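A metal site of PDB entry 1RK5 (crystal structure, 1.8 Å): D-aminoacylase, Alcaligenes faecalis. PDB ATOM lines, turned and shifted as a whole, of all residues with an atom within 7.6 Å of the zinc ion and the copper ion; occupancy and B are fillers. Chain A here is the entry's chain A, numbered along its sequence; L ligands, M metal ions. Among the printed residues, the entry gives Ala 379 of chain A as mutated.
O1 of the ligand binds the zinc ion, at 2.0 Å. ND1 of His 233 binds the zinc ion (2.1 Å). The zinc ion is bound by a ring nitrogen (NE2) of His 263, 2.2 Å away. The side-chain sulfur (SG) of Cys 109 is bound to the zinc ion (2.3 Å). Slightly farther from the zinc ion lies an oxygen (O2) of the ligand (2.7 Å).
Asn 108 touches the copper ion. Within 4 Å of the copper ion: His 80, His 82, Asn 108 and Cys 109. The nearest printed residue that does not touch the copper ion is His 263 (4.2 Å).
The copper ion is bound by a ring nitrogen (NE2) of His 82, a ring nitrogen (NE2) of His 80, the side-chain sulfur (SG) of Cys 109 and an oxygen (O2) of the ligand. The copper ion has four donor atoms within binding distance.
O of Thr 201 lies within hydrogen-bond range of N of His 233, at 3.0 Å. O of His 80 is in hydrogen-bond range of N of Ala 379, at 2.7 Å. A ring nitrogen (ND1) of His 80 lies close to the side-chain hydroxyl (OG) of Ser 262 (3.4 Å). A ring nitrogen (ND1) of His 263 is in hydrogen-bond range of the side-chain carboxylate of Glu 237, at 3.1 Å. The side-chain amino group (NZ) of Lys 265 lies within hydrogen-bond range of the backbone carbonyl oxygen (O) of His 263 (3.0 Å). The side-chain amide oxygen (OD1) of Asn 108 lies close to the backbone carbonyl oxygen (O) of Thr 81, at 3.0 Å.
Of the 27 residues printed, 3 come within 4 Å of the zinc ion. The nearest printed residue that does not touch the zinc ion is Tyr 205 (4.05 Å).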
ATOM      1  N   HIS A  80      27.363 -31.417 -21.451  1.00  0.00           N
ATOM      2  CA  HIS A  80      27.471 -29.988 -21.142  1.00  0.00           C
ATOM      3  C   HIS A  80      27.982 -29.715 -19.732  1.00  0.00           C
ATOM      4  O   HIS A  80      27.203 -29.694 -18.784  1.00  0.00           O
ATOM      5  CB  HIS A  80      26.113 -29.307 -21.307  1.00  0.00           C
ATOM      6  CG  HIS A  80      26.215 -27.808 -21.334  1.00  0.00           C
ATOM      7  ND1 HIS A  80      26.361 -27.098 -22.503  1.00  0.00           N
ATOM      8  CD2 HIS A  80      26.259 -26.903 -20.326  1.00  0.00           C
ATOM      9  CE1 HIS A  80      26.499 -25.808 -22.211  1.00  0.00           C
ATOM     10  NE2 HIS A  80      26.441 -25.673 -20.898  1.00  0.00           N
ATOM     11  N   THR A  81      29.282 -29.496 -19.603  1.00  0.00           N
ATOM     12  CA  THR A  81      29.862 -29.231 -18.296  1.00  0.00           C
ATOM     13  C   THR A  81      30.671 -27.937 -18.263  1.00  0.00           C
ATOM     14  O   THR A  81      31.049 -27.374 -19.295  1.00  0.00           O
ATOM     15  CB  THR A  81      30.833 -30.344 -17.836  1.00  0.00           C
ATOM     16  OG1 THR A  81      32.125 -30.115 -18.425  1.00  0.00           O
ATOM     17  CG2 THR A  81      30.338 -31.722 -18.268  1.00  0.00           C
ATOM     18  N   HIS A  82      30.924 -27.476 -17.043  1.00  0.00           N
ATOM     19  CA  HIS A  82      31.739 -26.300 -16.794  1.00  0.00           C
ATOM     20  C   HIS A  82      32.771 -26.788 -15.787  1.00  0.00           C
ATOM     21  O   HIS A  82      33.055 -26.138 -14.779  1.00  0.00           O
ATOM     22  CB  HIS A  82      30.890 -25.171 -16.205  1.00  0.00           C
ATOM     23  CG  HIS A  82      29.932 -24.588 -17.191  1.00  0.00           C
ATOM     24  ND1 HIS A  82      30.357 -23.879 -18.304  1.00  0.00           N
ATOM     25  CD2 HIS A  82      28.584 -24.654 -17.280  1.00  0.00           C
ATOM     26  CE1 HIS A  82      29.309 -23.549 -19.033  1.00  0.00           C
ATOM     27  NE2 HIS A  82      28.225 -24.004 -18.442  1.00  0.00           N
ATOM     28  N   GLY A 107      34.530 -26.449 -21.615  1.00  0.00           N
ATOM     29  CA  GLY A 107      34.615 -25.210 -22.379  1.00  0.00           C
ATOM     30  C   GLY A 107      33.350 -24.822 -23.115  1.00  0.00           C
ATOM     31  O   GLY A 107      33.376 -24.519 -24.307  1.00  0.00           O
ATOM     32  N   ASN A 108      32.223 -24.813 -22.392  1.00  0.00           N
ATOM     33  CA  ASN A 108      30.938 -24.488 -22.984  1.00  0.00           C
ATOM     34  C   ASN A 108      30.474 -23.039 -22.835  1.00  0.00           C
ATOM     35  O   ASN A 108      31.016 -22.271 -22.033  1.00  0.00           O
ATOM     36  CB  ASN A 108      29.865 -25.421 -22.408  1.00  0.00           C
ATOM     37  CG  ASN A 108      30.002 -26.845 -22.919  1.00  0.00           C
ATOM     38  OD1 ASN A 108      30.514 -27.731 -22.222  1.00  0.00           O
ATOM     39  ND2 ASN A 108      29.558 -27.064 -24.142  1.00  0.00           N
ATOM     40  N   CYS A 109      29.468 -22.678 -23.632  1.00  0.00           N
ATOM     41  CA  CYS A 109      28.849 -21.357 -23.608  1.00  0.00           C
ATOM     42  C   CYS A 109      29.835 -20.203 -23.793  1.00  0.00           C
ATOM     43  O   CYS A 109      29.616 -19.110 -23.272  1.00  0.00           O
ATOM     44  CB  CYS A 109      28.061 -21.192 -22.312  1.00  0.00           C
ATOM     45  SG  CYS A 109      26.877 -22.552 -22.010  1.00  0.00           S
ATOM     46  N   GLY A 110      30.910 -20.460 -24.528  1.00  0.00           N
ATOM     47  CA  GLY A 110      31.923 -19.451 -24.790  1.00  0.00           C
ATOM     48  C   GLY A 110      32.914 -19.291 -23.643  1.00  0.00           C
ATOM     49  O   GLY A 110      33.823 -18.473 -23.724  1.00  0.00           O
ATOM     50  N   ILE A 111      32.730 -20.090 -22.592  1.00  0.00           N
ATOM     51  CA  ILE A 111      33.579 -20.030 -21.402  1.00  0.00           C
ATOM     52  C   ILE A 111      34.559 -21.195 -21.242  1.00  0.00           C
ATOM     53  O   ILE A 111      34.155 -22.290 -20.865  1.00  0.00           O
ATOM     54  CB  ILE A 111      32.710 -20.004 -20.121  1.00  0.00           C
ATOM     55  CG1 ILE A 111      31.689 -18.870 -20.213  1.00  0.00           C
ATOM     56  CG2 ILE A 111      33.590 -19.840 -18.900  1.00  0.00           C
ATOM     57  CD1 ILE A 111      30.565 -18.998 -19.198  1.00  0.00           C
ATOM     58  N   LEU A 127      32.797 -18.050 -13.128  1.00  0.00           N
ATOM     59  CA  LEU A 127      32.132 -19.257 -12.639  1.00  0.00           C
ATOM     60  C   LEU A 127      33.133 -20.412 -12.518  1.00  0.00           C
ATOM     61  O   LEU A 127      32.878 -21.385 -11.801  1.00  0.00           O
ATOM     62  CB  LEU A 127      30.978 -19.656 -13.564  1.00  0.00           C
ATOM     63  CG  LEU A 127      29.710 -18.802 -13.509  1.00  0.00           C
ATOM     64  CD1 LEU A 127      28.744 -19.259 -14.590  1.00  0.00           C
ATOM     65  CD2 LEU A 127      29.072 -18.926 -12.122  1.00  0.00           C
ATOM     66  N   THR A 201      30.338 -20.662 -28.053  1.00  0.00           N
ATOM     67  CA  THR A 201      30.020 -19.239 -27.920  1.00  0.00           C
ATOM     68  C   THR A 201      28.875 -19.047 -26.931  1.00  0.00           C
ATOM     69  O   THR A 201      28.106 -19.972 -26.644  1.00  0.00           O
ATOM     70  CB  THR A 201      29.560 -18.618 -29.253  1.00  0.00           C
ATOM     71  OG1 THR A 201      28.350 -19.246 -29.686  1.00  0.00           O
ATOM     72  CG2 THR A 201      30.631 -18.771 -30.331  1.00  0.00           C
ATOM     73  N   GLY A 202      28.759 -17.822 -26.414  1.00  0.00           N
ATOM     74  CA  GLY A 202      27.699 -17.486 -25.480  1.00  0.00           C
ATOM     75  C   GLY A 202      27.404 -15.998 -25.594  1.00  0.00           C
ATOM     76  O   GLY A 202      27.638 -15.233 -24.655  1.00  0.00           O
ATOM     77  N   PHE A 204      24.871 -14.488 -25.320  1.00  0.00           N
ATOM     78  CA  PHE A 204      23.851 -14.077 -24.351  1.00  0.00           C
ATOM     79  C   PHE A 204      24.518 -13.261 -23.241  1.00  0.00           C
ATOM     80  O   PHE A 204      23.916 -12.347 -22.686  1.00  0.00           O
ATOM     81  CB  PHE A 204      23.189 -15.318 -23.744  1.00  0.00           C
ATOM     82  CG  PHE A 204      22.347 -15.034 -22.525  1.00  0.00           C
ATOM     83  CD1 PHE A 204      21.093 -14.443 -22.645  1.00  0.00           C
ATOM     84  CD2 PHE A 204      22.808 -15.383 -21.254  1.00  0.00           C
ATOM     85  CE1 PHE A 204      20.301 -14.186 -21.512  1.00  0.00           C
ATOM     86  CE2 PHE A 204      22.034 -15.137 -20.114  1.00  0.00           C
ATOM     87  CZ  PHE A 204      20.776 -14.539 -20.255  1.00  0.00           C
ATOM     88  N   TYR A 205      25.768 -13.585 -22.937  1.00  0.00           N
ATOM     89  CA  TYR A 205      26.505 -12.925 -21.857  1.00  0.00           C
ATOM     90  C   TYR A 205      27.243 -11.639 -22.220  1.00  0.00           C
ATOM     91  O   TYR A 205      27.632 -11.420 -23.379  1.00  0.00           O
ATOM     92  CB  TYR A 205      27.472 -13.937 -21.240  1.00  0.00           C
ATOM     93  CG  TYR A 205      26.784 -15.122 -20.574  1.00  0.00           C
ATOM     94  CD1 TYR A 205      26.016 -14.953 -19.420  1.00  0.00           C
ATOM     95  CD2 TYR A 205      26.909 -16.405 -21.108  1.00  0.00           C
ATOM     96  CE1 TYR A 205      25.405 -16.040 -18.791  1.00  0.00           C
ATOM     97  CE2 TYR A 205      26.287 -17.496 -20.488  1.00  0.00           C
ATOM     98  CZ  TYR A 205      25.543 -17.314 -19.343  1.00  0.00           C
ATOM     99  OH  TYR A 205      24.965 -18.397 -18.709  1.00  0.00           O
ATOM    100  N   THR A 232      26.853 -23.883 -28.761  1.00  0.00           N
ATOM    101  CA  THR A 232      26.384 -22.543 -28.410  1.00  0.00           C
ATOM    102  C   THR A 232      25.276 -22.371 -27.376  1.00  0.00           C
ATOM    103  O   THR A 232      24.324 -23.149 -27.321  1.00  0.00           O
ATOM    104  CB  THR A 232      25.911 -21.794 -29.674  1.00  0.00           C
ATOM    105  OG1 THR A 232      25.359 -20.520 -29.303  1.00  0.00           O
ATOM    106  CG2 THR A 232      24.834 -22.587 -30.408  1.00  0.00           C
ATOM    107  N   HIS A 233      25.451 -21.344 -26.559  1.00  0.00           N
ATOM    108  CA  HIS A 233      24.443 -20.941 -25.590  1.00  0.00           C
ATOM    109  C   HIS A 233      23.880 -19.809 -26.455  1.00  0.00           C
ATOM    110  O   HIS A 233      24.489 -18.742 -26.565  1.00  0.00           O
ATOM    111  CB  HIS A 233      25.099 -20.383 -24.316  1.00  0.00           C
ATOM    112  CG  HIS A 233      24.127 -19.776 -23.353  1.00  0.00           C
ATOM    113  ND1 HIS A 233      24.253 -19.940 -21.983  1.00  0.00           N
ATOM    114  CD2 HIS A 233      23.047 -18.981 -23.541  1.00  0.00           C
ATOM    115  CE1 HIS A 233      23.279 -19.271 -21.378  1.00  0.00           C
ATOM    116  NE2 HIS A 233      22.540 -18.682 -22.300  1.00  0.00           N
ATOM    117  N   MET A 234      22.745 -20.061 -27.094  1.00  0.00           N
ATOM    118  CA  MET A 234      22.148 -19.084 -28.008  1.00  0.00           C
ATOM    119  C   MET A 234      22.007 -17.678 -27.421  1.00  0.00           C
ATOM    120  O   MET A 234      21.940 -17.502 -26.203  1.00  0.00           O
ATOM    121  CB  MET A 234      20.810 -19.609 -28.530  1.00  0.00           C
ATOM    122  CG  MET A 234      20.953 -20.967 -29.215  1.00  0.00           C
ATOM    123  SD  MET A 234      19.508 -21.582 -30.102  1.00  0.00           S
ATOM    124  CE  MET A 234      18.396 -21.965 -28.723  1.00  0.00           C
ATOM    125  N   GLU A 237      17.039 -17.128 -25.246  1.00  0.00           N
ATOM    126  CA  GLU A 237      16.268 -18.360 -25.109  1.00  0.00           C
ATOM    127  C   GLU A 237      14.828 -18.074 -24.674  1.00  0.00           C
ATOM    128  O   GLU A 237      14.165 -18.945 -24.101  1.00  0.00           O
ATOM    129  CB  GLU A 237      16.931 -19.302 -24.107  1.00  0.00           C
ATOM    130  CG  GLU A 237      18.316 -19.796 -24.526  1.00  0.00           C
ATOM    131  CD  GLU A 237      18.920 -20.787 -23.526  1.00  0.00           C
ATOM    132  OE1 GLU A 237      19.070 -20.414 -22.343  1.00  0.00           O
ATOM    133  OE2 GLU A 237      19.231 -21.928 -23.922  1.00  0.00           O
ATOM    134  N   SER A 262      23.140 -25.841 -26.860  1.00  0.00           N
ATOM    135  CA  SER A 262      23.276 -26.151 -25.439  1.00  0.00           C
ATOM    136  C   SER A 262      22.030 -25.913 -24.597  1.00  0.00           C
ATOM    137  O   SER A 262      21.273 -24.962 -24.831  1.00  0.00           O
ATOM    138  CB  SER A 262      24.429 -25.340 -24.838  1.00  0.00           C
ATOM    139  OG  SER A 262      25.662 -25.659 -25.479  1.00  0.00           O
ATOM    140  N   HIS A 263      21.837 -26.774 -23.596  1.00  0.00           N
ATOM    141  CA  HIS A 263      20.719 -26.698 -22.663  1.00  0.00           C
ATOM    142  C   HIS A 263      19.464 -26.047 -23.228  1.00  0.00           C
ATOM    143  O   HIS A 263      19.051 -24.974 -22.771  1.00  0.00           O
ATOM    144  CB  HIS A 263      21.159 -25.974 -21.366  1.00  0.00           C
ATOM    145  CG  HIS A 263      21.885 -24.677 -21.613  1.00  0.00           C
ATOM    146  ND1 HIS A 263      21.350 -23.641 -22.347  1.00  0.00           N
ATOM    147  CD2 HIS A 263      23.090 -24.238 -21.160  1.00  0.00           C
ATOM    148  CE1 HIS A 263      22.186 -22.612 -22.329  1.00  0.00           C
ATOM    149  NE2 HIS A 263      23.251 -22.956 -21.623  1.00  0.00           N
ATOM    150  N   LYS A 265      15.823 -24.840 -23.978  1.00  0.00           N
ATOM    151  CA  LYS A 265      14.703 -24.482 -23.097  1.00  0.00           C
ATOM    152  C   LYS A 265      13.951 -23.291 -23.674  1.00  0.00           C
ATOM    153  O   LYS A 265      14.392 -22.654 -24.633  1.00  0.00           O
ATOM    154  CB  LYS A 265      15.255 -24.043 -21.736  1.00  0.00           C
ATOM    155  CG  LYS A 265      15.987 -22.685 -21.831  1.00  0.00           C
ATOM    156  CD  LYS A 265      16.401 -22.114 -20.474  1.00  0.00           C
ATOM    157  CE  LYS A 265      17.571 -22.880 -19.877  1.00  0.00           C
ATOM    158  NZ  LYS A 265      18.843 -22.755 -20.693  1.00  0.00           N
ATOM    159  N   TYR A 296      19.116 -30.424 -19.489  1.00  0.00           N
ATOM    160  CA  TYR A 296      19.161 -30.981 -18.136  1.00  0.00           C
ATOM    161  C   TYR A 296      17.711 -31.135 -17.689  1.00  0.00           C
ATOM    162  O   TYR A 296      16.842 -30.371 -18.091  1.00  0.00           O
ATOM    163  CB  TYR A 296      19.984 -30.074 -17.200  1.00  0.00           C
ATOM    164  CG  TYR A 296      19.613 -28.620 -17.206  1.00  0.00           C
ATOM    165  CD1 TYR A 296      18.496 -28.156 -16.514  1.00  0.00           C
ATOM    166  CD2 TYR A 296      20.392 -27.687 -17.897  1.00  0.00           C
ATOM    167  CE1 TYR A 296      18.164 -26.808 -16.507  1.00  0.00           C
ATOM    168  CE2 TYR A 296      20.071 -26.333 -17.895  1.00  0.00           C
ATOM    169  CZ  TYR A 296      18.959 -25.905 -17.202  1.00  0.00           C
ATOM    170  OH  TYR A 296      18.647 -24.566 -17.203  1.00  0.00           O
ATOM    171  N   SER A 302      20.654 -21.811 -13.898  1.00  0.00           N
ATOM    172  CA  SER A 302      21.657 -21.273 -12.978  1.00  0.00           C
ATOM    173  C   SER A 302      22.871 -20.759 -13.744  1.00  0.00           C
ATOM    174  O   SER A 302      23.339 -21.393 -14.694  1.00  0.00           O
ATOM    175  CB  SER A 302      22.080 -22.347 -11.966  1.00  0.00           C
ATOM    176  OG  SER A 302      22.976 -21.813 -10.994  1.00  0.00           O
ATOM    177  N   THR A 303      23.376 -19.603 -13.326  1.00  0.00           N
ATOM    178  CA  THR A 303      24.546 -18.988 -13.947  1.00  0.00           C
ATOM    179  C   THR A 303      24.898 -17.734 -13.157  1.00  0.00           C
ATOM    180  O   THR A 303      24.532 -17.608 -11.985  1.00  0.00           O
ATOM    181  CB  THR A 303      24.261 -18.628 -15.434  1.00  0.00           C
ATOM    182  OG1 THR A 303      25.446 -18.043 -16.015  1.00  0.00           O
ATOM    183  CG2 THR A 303      23.102 -17.647 -15.551  1.00  0.00           C
ATOM    184  N   ALA A 379      25.165 -29.216 -17.009  1.00  0.00           N
ATOM    185  CA  ALA A 379      25.372 -27.771 -16.867  1.00  0.00           C
ATOM    186  C   ALA A 379      25.700 -27.448 -15.411  1.00  0.00           C
ATOM    187  O   ALA A 379      25.434 -26.356 -14.925  1.00  0.00           O
ATOM    188  CB  ALA A 379      24.121 -27.002 -17.314  1.00  0.00           C
ATOM    189  N   GLY A 380      26.268 -28.425 -14.704  1.00  0.00           N
ATOM    190  CA  GLY A 380      26.630 -28.206 -13.316  1.00  0.00           C
ATOM    191  C   GLY A 380      27.684 -27.124 -13.144  1.00  0.00           C
ATOM    192  O   GLY A 380      28.569 -26.974 -13.987  1.00  0.00           O
ATOM    193  N   LEU A 381      27.582 -26.356 -12.072  1.00  0.00           N
ATOM    194  CA  LEU A 381      28.538 -25.290 -11.777  1.00  0.00           C
ATOM    195  C   LEU A 381      29.169 -25.741 -10.462  1.00  0.00           C
ATOM    196  O   LEU A 381      28.728 -25.368  -9.366  1.00  0.00           O
ATOM    197  CB  LEU A 381      27.794 -23.945 -11.640  1.00  0.00           C
ATOM    198  CG  LEU A 381      27.025 -23.572 -12.914  1.00  0.00           C
ATOM    199  CD1 LEU A 381      26.210 -22.299 -12.713  1.00  0.00           C
ATOM    200  CD2 LEU A 381      28.019 -23.376 -14.055  1.00  0.00           C
ATOM    201  N   ARG A 390      21.404 -30.069 -10.162  1.00  0.00           N
ATOM    202  CA  ARG A 390      21.710 -30.745 -11.416  1.00  0.00           C
ATOM    203  C   ARG A 390      23.165 -31.217 -11.401  1.00  0.00           C
ATOM    204  O   ARG A 390      23.524 -32.214 -12.038  1.00  0.00           O
ATOM    205  CB  ARG A 390      21.470 -29.813 -12.609  1.00  0.00           C
ATOM    206  CG  ARG A 390      22.372 -28.587 -12.681  1.00  0.00           C
ATOM    207  CD  ARG A 390      21.783 -27.553 -13.648  1.00  0.00           C
ATOM    208  NE  ARG A 390      22.698 -26.458 -13.948  1.00  0.00           N
ATOM    209  CZ  ARG A 390      22.349 -25.324 -14.546  1.00  0.00           C
ATOM    210  NH1 ARG A 390      21.088 -25.129 -14.914  1.00  0.00           N
ATOM    211  NH2 ARG A 390      23.262 -24.399 -14.816  1.00  0.00           N
HETATM  212  C1  LIG L   1      25.410 -21.920 -18.494  1.00  0.00           C
HETATM  213  O1  LIG L   1      25.330 -20.948 -19.281  1.00  0.00           O
HETATM  214  O2  LIG L   1      25.177 -23.103 -18.826  1.00  0.00           O
HETATM  215  C2  LIG L   1      25.973 -21.655 -17.115  1.00  0.00           C
HETATM  216 ZN    ZN M   1      24.968 -21.673 -21.083  1.00  0.00          ZN
HETATM  217 CU    CU M   2      27.187 -23.847 -20.156  1.00  0.00          CU
